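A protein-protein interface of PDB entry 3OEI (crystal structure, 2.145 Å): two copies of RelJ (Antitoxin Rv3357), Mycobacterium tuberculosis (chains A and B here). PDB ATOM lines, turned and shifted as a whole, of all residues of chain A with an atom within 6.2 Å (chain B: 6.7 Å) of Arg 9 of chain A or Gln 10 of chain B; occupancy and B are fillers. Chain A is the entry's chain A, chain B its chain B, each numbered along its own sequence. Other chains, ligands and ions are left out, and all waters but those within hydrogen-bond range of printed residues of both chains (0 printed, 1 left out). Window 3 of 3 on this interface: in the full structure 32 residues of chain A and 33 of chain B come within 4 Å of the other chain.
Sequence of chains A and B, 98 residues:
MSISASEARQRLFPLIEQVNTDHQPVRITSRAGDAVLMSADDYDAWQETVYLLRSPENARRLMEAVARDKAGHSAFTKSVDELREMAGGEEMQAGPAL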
ATOM      1  N   SER A   4       2.397  21.232   3.164  1.00  0.00           N
ATOM      2  CA  SER A   4       3.161  21.322   1.924  1.00  0.00           C
ATOM      3  C   SER A   4       4.629  21.037   2.199  1.00  0.00           C
ATOM      4  O   SER A   4       5.115  21.247   3.312  1.00  0.00           O
ATOM      5  CB  SER A   4       3.048  22.732   1.326  1.00  0.00           C
ATOM      6  OG  SER A   4       3.871  23.628   2.067  1.00  0.00           O
ATOM      7  N   ALA A   5       5.346  20.601   1.170  1.00  0.00           N
ATOM      8  CA  ALA A   5       6.767  20.266   1.310  1.00  0.00           C
ATOM      9  C   ALA A   5       7.576  21.472   1.756  1.00  0.00           C
ATOM     10  O   ALA A   5       8.585  21.344   2.436  1.00  0.00           O
ATOM     11  CB  ALA A   5       7.313  19.720   0.001  1.00  0.00           C
ATOM     12  N   SER A   6       7.126  22.654   1.364  1.00  0.00           N
ATOM     13  CA  SER A   6       7.848  23.854   1.720  1.00  0.00           C
ATOM     14  C   SER A   6       7.846  24.122   3.228  1.00  0.00           C
ATOM     15  O   SER A   6       8.876  24.462   3.798  1.00  0.00           O
ATOM     16  CB  SER A   6       7.308  25.049   0.938  1.00  0.00           C
ATOM     17  OG  SER A   6       8.184  26.141   1.083  1.00  0.00           O
ATOM     18  N   GLU A   7       6.705  23.965   3.887  1.00  0.00           N
ATOM     19  CA  GLU A   7       6.682  24.161   5.344  1.00  0.00           C
ATOM     20  C   GLU A   7       7.336  23.003   6.104  1.00  0.00           C
ATOM     21  O   GLU A   7       7.965  23.196   7.150  1.00  0.00           O
ATOM     22  CB  GLU A   7       5.270  24.433   5.857  1.00  0.00           C
ATOM     23  CG  GLU A   7       4.163  23.622   5.198  1.00  0.00           C
ATOM     24  CD  GLU A   7       2.767  24.109   5.611  1.00  0.00           C
ATOM     25  OE1 GLU A   7       2.558  24.329   6.835  1.00  0.00           O
ATOM     26  OE2 GLU A   7       1.895  24.292   4.718  1.00  0.00           O
ATOM     27  N   ALA A   8       7.214  21.804   5.557  1.00  0.00           N
ATOM     28  CA  ALA A   8       7.788  20.629   6.193  1.00  0.00           C
ATOM     29  C   ALA A   8       9.295  20.745   6.229  1.00  0.00           C
ATOM     30  O   ALA A   8       9.945  20.295   7.178  1.00  0.00           O
ATOM     31  CB  ALA A   8       7.358  19.339   5.449  1.00  0.00           C
ATOM     32  N   ARG A   9       9.862  21.349   5.190  1.00  0.00           N
ATOM     33  CA  ARG A   9      11.303  21.528   5.149  1.00  0.00           C
ATOM     34  C   ARG A   9      11.743  22.566   6.190  1.00  0.00           C
ATOM     35  O   ARG A   9      12.713  22.362   6.915  1.00  0.00           O
ATOM     36  CB  ARG A   9      11.739  21.938   3.742  1.00  0.00           C
ATOM     37  CG  ARG A   9      13.170  22.395   3.658  1.00  0.00           C
ATOM     38  CD  ARG A   9      13.594  22.596   2.202  1.00  0.00           C
ATOM     39  NE  ARG A   9      15.040  22.478   2.053  1.00  0.00           N
ATOM     40  CZ  ARG A   9      15.797  23.418   1.501  1.00  0.00           C
ATOM     41  NH1 ARG A   9      15.233  24.540   1.062  1.00  0.00           N
ATOM     42  NH2 ARG A   9      17.110  23.240   1.397  1.00  0.00           N
ATOM     43  N   GLN A  10      11.017  23.667   6.276  1.00  0.00           N
ATOM     44  CA  GLN A  10      11.306  24.686   7.283  1.00  0.00           C
ATOM     45  C   GLN A  10      11.161  24.133   8.696  1.00  0.00           C
ATOM     46  O   GLN A  10      11.973  24.412   9.579  1.00  0.00           O
ATOM     47  CB  GLN A  10      10.356  25.878   7.127  1.00  0.00           C
ATOM     48  CG  GLN A  10      10.710  26.848   6.017  1.00  0.00           C
ATOM     49  CD  GLN A  10       9.593  27.842   5.764  1.00  0.00           C
ATOM     50  OE1 GLN A  10       9.690  29.013   6.131  1.00  0.00           O
ATOM     51  NE2 GLN A  10       8.515  27.374   5.146  1.00  0.00           N
ATOM     52  N   ARG A  11      10.136  23.315   8.898  1.00  0.00           N
ATOM     53  CA  ARG A  11       9.767  22.858  10.235  1.00  0.00           C
ATOM     54  C   ARG A  11      10.114  21.390  10.483  1.00  0.00           C
ATOM     55  O   ARG A  11       9.538  20.752  11.376  1.00  0.00           O
ATOM     56  CB  ARG A  11       8.263  23.059  10.452  1.00  0.00           C
ATOM     57  CG  ARG A  11       7.798  24.501  10.298  1.00  0.00           C
ATOM     58  CD  ARG A  11       8.602  25.480  11.197  1.00  0.00           C
ATOM     59  NE  ARG A  11       8.197  26.835  10.835  1.00  0.00           N
ATOM     60  CZ  ARG A  11       9.017  27.813  10.499  1.00  0.00           C
ATOM     61  NH1 ARG A  11       8.503  28.984  10.167  1.00  0.00           N
ATOM     62  NH2 ARG A  11      10.334  27.637  10.528  1.00  0.00           N
ATOM     63  N   LEU A  12      11.044  20.839   9.710  1.00  0.00           N
ATOM     64  CA  LEU A  12      11.309  19.397   9.840  1.00  0.00           C
ATOM     65  C   LEU A  12      11.669  18.982  11.271  1.00  0.00           C
ATOM     66  O   LEU A  12      11.204  17.963  11.764  1.00  0.00           O
ATOM     67  CB  LEU A  12      12.378  18.918   8.846  1.00  0.00           C
ATOM     68  CG  LEU A  12      12.513  17.391   8.852  1.00  0.00           C
ATOM     69  CD1 LEU A  12      11.181  16.799   8.487  1.00  0.00           C
ATOM     70  CD2 LEU A  12      13.630  16.873   7.923  1.00  0.00           C
ATOM     71  N   PHE A  13      12.497  19.773  11.947  1.00  0.00           N
ATOM     72  CA  PHE A  13      12.937  19.387  13.279  1.00  0.00           C
ATOM     73  C   PHE A  13      11.797  19.195  14.304  1.00  0.00           C
ATOM     74  O   PHE A  13      11.708  18.138  14.939  1.00  0.00           O
ATOM     75  CB  PHE A  13      14.030  20.333  13.809  1.00  0.00           C
ATOM     76  CG  PHE A  13      15.333  20.237  13.060  1.00  0.00           C
ATOM     77  CD1 PHE A  13      15.440  19.457  11.913  1.00  0.00           C
ATOM     78  CD2 PHE A  13      16.457  20.922  13.508  1.00  0.00           C
ATOM     79  CE1 PHE A  13      16.636  19.366  11.230  1.00  0.00           C
ATOM     80  CE2 PHE A  13      17.658  20.831  12.827  1.00  0.00           C
ATOM     81  CZ  PHE A  13      17.751  20.049  11.689  1.00  0.00           C
ATOM     82  N   LEU A  15       8.751  18.791  13.624  1.00  0.00           N
ATOM     83  CA  LEU A  15       7.843  17.766  13.101  1.00  0.00           C
ATOM     84  C   LEU A  15       8.337  16.349  13.454  1.00  0.00           C
ATOM     85  O   LEU A  15       7.540  15.460  13.692  1.00  0.00           O
ATOM     86  CB  LEU A  15       7.602  17.932  11.604  1.00  0.00           C
ATOM     87  CG  LEU A  15       6.712  19.114  11.191  1.00  0.00           C
ATOM     88  CD1 LEU A  15       6.761  19.252   9.684  1.00  0.00           C
ATOM     89  CD2 LEU A  15       5.256  18.967  11.690  1.00  0.00           C
ATOM     90  N   ALA B   5      18.959  14.597  10.589  1.00  0.00           N
ATOM     91  CA  ALA B   5      17.812  15.461  10.389  1.00  0.00           C
ATOM     92  C   ALA B   5      18.277  16.707   9.640  1.00  0.00           C
ATOM     93  O   ALA B   5      17.516  17.299   8.893  1.00  0.00           O
ATOM     94  CB  ALA B   5      17.169  15.813  11.717  1.00  0.00           C
ATOM     95  N   SER B   6      19.544  17.071   9.840  1.00  0.00           N
ATOM     96  CA  SER B   6      20.156  18.227   9.180  1.00  0.00           C
ATOM     97  C   SER B   6      20.198  18.030   7.663  1.00  0.00           C
ATOM     98  O   SER B   6      19.657  18.827   6.898  1.00  0.00           O
ATOM     99  CB  SER B   6      21.576  18.462   9.734  1.00  0.00           C
ATOM    100  OG  SER B   6      22.215  19.518   9.054  1.00  0.00           O
ATOM    101  N   GLU B   7      20.839  16.953   7.245  1.00  0.00           N
ATOM    102  CA  GLU B   7      20.817  16.521   5.854  1.00  0.00           C
ATOM    103  C   GLU B   7      19.389  16.310   5.311  1.00  0.00           C
ATOM    104  O   GLU B   7      19.067  16.758   4.216  1.00  0.00           O
ATOM    105  CB  GLU B   7      21.648  15.233   5.685  1.00  0.00           C
ATOM    106  CG  GLU B   7      21.603  14.644   4.271  1.00  0.00           C
ATOM    107  CD  GLU B   7      22.674  13.588   4.038  1.00  0.00           C
ATOM    108  OE1 GLU B   7      23.479  13.355   4.963  1.00  0.00           O
ATOM    109  OE2 GLU B   7      22.707  12.982   2.937  1.00  0.00           O
ATOM    110  N   ALA B   8      18.531  15.634   6.069  1.00  0.00           N
ATOM    111  CA  ALA B   8      17.176  15.387   5.582  1.00  0.00           C
ATOM    112  C   ALA B   8      16.446  16.690   5.292  1.00  0.00           C
ATOM    113  O   ALA B   8      15.788  16.820   4.276  1.00  0.00           O
ATOM    114  CB  ALA B   8      16.362  14.518   6.569  1.00  0.00           C
ATOM    115  N   ARG B   9      16.575  17.661   6.185  1.00  0.00           N
ATOM    116  CA  ARG B   9      15.892  18.921   5.994  1.00  0.00           C
ATOM    117  C   ARG B   9      16.461  19.688   4.785  1.00  0.00           C
ATOM    118  O   ARG B   9      15.713  20.213   3.953  1.00  0.00           O
ATOM    119  CB  ARG B   9      15.949  19.761   7.270  1.00  0.00           C
ATOM    120  CG  ARG B   9      15.312  21.132   7.077  1.00  0.00           C
ATOM    121  CD  ARG B   9      15.394  21.949   8.324  1.00  0.00           C
ATOM    122  NE  ARG B   9      16.771  22.252   8.655  1.00  0.00           N
ATOM    123  CZ  ARG B   9      17.140  23.009   9.681  1.00  0.00           C
ATOM    124  NH1 ARG B   9      16.216  23.556  10.469  1.00  0.00           N
ATOM    125  NH2 ARG B   9      18.430  23.233   9.912  1.00  0.00           N
ATOM    126  N   GLN B  10      17.783  19.744   4.696  1.00  0.00           N
ATOM    127  CA  GLN B  10      18.440  20.316   3.524  1.00  0.00           C
ATOM    128  C   GLN B  10      17.922  19.723   2.193  1.00  0.00           C
ATOM    129  O   GLN B  10      17.672  20.454   1.230  1.00  0.00           O
ATOM    130  CB  GLN B  10      19.952  20.117   3.625  1.00  0.00           C
ATOM    131  CG  GLN B  10      20.683  20.548   2.367  1.00  0.00           C
ATOM    132  CD  GLN B  10      20.487  22.022   2.088  1.00  0.00           C
ATOM    133  OE1 GLN B  10      20.551  22.853   3.009  1.00  0.00           O
ATOM    134  NE2 GLN B  10      20.233  22.363   0.819  1.00  0.00           N
ATOM    135  N   ARG B  11      17.727  18.411   2.149  1.00  0.00           N
ATOM    136  CA  ARG B  11      17.439  17.734   0.881  1.00  0.00           C
ATOM    137  C   ARG B  11      15.979  17.311   0.745  1.00  0.00           C
ATOM    138  O   ARG B  11      15.646  16.429  -0.069  1.00  0.00           O
ATOM    139  CB  ARG B  11      18.305  16.479   0.742  1.00  0.00           C
ATOM    140  CG  ARG B  11      19.807  16.683   0.925  1.00  0.00           C
ATOM    141  CD  ARG B  11      20.490  15.315   1.035  1.00  0.00           C
ATOM    142  NE  ARG B  11      19.985  14.431  -0.007  1.00  0.00           N
ATOM    143  CZ  ARG B  11      19.924  13.105   0.067  1.00  0.00           C
ATOM    144  NH1 ARG B  11      20.366  12.455   1.142  1.00  0.00           N
ATOM    145  NH2 ARG B  11      19.426  12.424  -0.958  1.00  0.00           N
ATOM    146  N   LEU B  12      15.102  17.918   1.531  1.00  0.00           N
ATOM    147  CA  LEU B  12      13.751  17.355   1.676  1.00  0.00           C
ATOM    148  C   LEU B  12      12.967  17.342   0.365  1.00  0.00           C
ATOM    149  O   LEU B  12      12.189  16.429   0.126  1.00  0.00           O
ATOM    150  CB  LEU B  12      12.964  18.086   2.776  1.00  0.00           C
ATOM    151  CG  LEU B  12      11.614  17.441   3.077  1.00  0.00           C
ATOM    152  CD1 LEU B  12      11.837  16.111   3.827  1.00  0.00           C
ATOM    153  CD2 LEU B  12      10.758  18.383   3.888  1.00  0.00           C
ATOM    154  N   PHE B  13      13.155  18.357  -0.488  1.00  0.00           N
ATOM    155  CA  PHE B  13      12.492  18.365  -1.784  1.00  0.00           C
ATOM    156  C   PHE B  13      12.899  17.161  -2.661  1.00  0.00           C
ATOM    157  O   PHE B  13      12.042  16.453  -3.186  1.00  0.00           O
ATOM    158  CB  PHE B  13      12.716  19.697  -2.549  1.00  0.00           C
ATOM    159  CG  PHE B  13      11.867  20.844  -2.042  1.00  0.00           C
ATOM    160  CD1 PHE B  13      10.505  20.875  -2.282  1.00  0.00           C
ATOM    161  CD2 PHE B  13      12.432  21.878  -1.309  1.00  0.00           C
ATOM    162  CE1 PHE B  13       9.717  21.932  -1.805  1.00  0.00           C
ATOM    163  CE2 PHE B  13      11.655  22.927  -0.834  1.00  0.00           C
ATOM    164  CZ  PHE B  13      10.290  22.945  -1.074  1.00  0.00           C
ATOM    165  N   PRO B  14      14.206  16.961  -2.874  1.00  0.00           N
ATOM    166  CA  PRO B  14      14.562  15.795  -3.687  1.00  0.00           C
ATOM    167  C   PRO B  14      14.324  14.467  -2.935  1.00  0.00           C
ATOM    168  O   PRO B  14      14.018  13.470  -3.602  1.00  0.00           O
ATOM    169  CB  PRO B  14      16.051  16.015  -3.998  1.00  0.00           C
ATOM    170  CG  PRO B  14      16.534  16.982  -2.959  1.00  0.00           C
ATOM    171  CD  PRO B  14      15.351  17.862  -2.666  1.00  0.00           C
ATOM    172  N   LEU B  15      14.425  14.457  -1.598  1.00  0.00           N
ATOM    173  CA  LEU B  15      14.096  13.235  -0.804  1.00  0.00           C
ATOM    174  C   LEU B  15      12.674  12.707  -1.010  1.00  0.00           C
ATOM    175  O   LEU B  15      12.460  11.499  -1.136  1.00  0.00           O
ATOM    176  CB  LEU B  15      14.327  13.454   0.688  1.00  0.00           C
ATOM    177  CG  LEU B  15      15.733  13.209   1.240  1.00  0.00           C
ATOM    178  CD1 LEU B  15      15.775  13.475   2.765  1.00  0.00           C
ATOM    179  CD2 LEU B  15      16.220  11.805   0.918  1.00  0.00           C
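The side-chain amide nitrogen (NE2) of Gln 10 of chain A is in hydrogen-bond range of the backbone carbonyl oxygen (O) of Ser 6 of chain A (3.2 Å).
The side-chain hydroxyl (OG) of Ser 4 of chain A lies close to the backbone NH (N) of Ser 6 of chain A, 3.5 Å away.
Among the printed residues, pairs that only touch across the chains: Phe 13 of chain A with Ala 5 of chain B, Arg 9 of chain A with Leu 12 of chain B, Leu 12 of chain A with Arg 9 of chain B, Arg 9 of chain A with Phe 13 of chain B, Phe 13 of chain A with Arg 9 of chain B, Ala 8 of chain A with Leu 12 of chain B, Ala 5 of chain A with Phe 13 of chain B, Ser 6 of chain A with Phe 13 of chain B, Leu 12 of chain A with Ala 8 of chain B, Phe 13 of chain A with Ser 6 of chain B and Ala 5 of chain A with Leu 12 of chain B.
Along chain A the printed residues that touch a printed residue of chain B span positions 5 to 13.
Hydrophobic or aromatic side chains of chain B within 4 Å of the printed part of chain A: Ala 5, Ala 8, Leu 12 and Phe 13.
Along chain B the printed residues that touch a printed residue of chain A span positions 5 to 13.
Among the printed residues, 13 pairs touch across the chains.
NE of Arg 9 of chain A lies within hydrogen-bond range of O of Arg 9 of chain B.
NH2 of Arg 9 of chain A lies within hydrogen-bond range of O of Gln 10 of chain B.
Ala 5 of chain A touches Leu 12 of chain B, but with the chains exchanged Leu 12 of chain A does not touch Ala 5 of chain B (4.03 Å).
Ala 5 of chain A touches Phe 13 of chain B, and with the chains exchanged Phe 13 of chain A touches Ala 5 of chain B.
Arg 9 of chain A touches Leu 12 of chain B, and with the chains exchanged Leu 12 of chain A touches Arg 9 of chain B.
Arg 9 of chain A touches Phe 13 of chain B, and with the chains exchanged Phe 13 of chain A touches Arg 9 of chain B.
Positions printed for both chains: 5, 6, 7, 8, 9, 10, 11, 12, 13 and 15.
Of the 13 pairs that touch across the chains among the printed residues, 11 have their exchanged pair printed and touching as well.
Of the printed residues of chain B, Arg 9 of chain A touches Arg 9, Gln 10, Leu 12 and Phe 13.
Of the printed residues of chain A, Ala 5 of chain B touches Phe 13 (3.2 Å).
Of the printed residues of chain A, Ser 6 of chain B touches Phe 13.
Gln 10 of chain B touches just one residue of chain A: Arg 9 (2.8 Å).
Printed residues of chain A within 4 Å of Phe 13 of chain B: Ala 5, Ser 6 and Arg 9.
The nearest residue of chain B that does not touch Arg 9 of chain A is Arg 11 of chain B (4.9 Å).
The nearest residue of chain A that does not touch Gln 10 of chain B is Leu 12 of chain A (6.0 Å).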
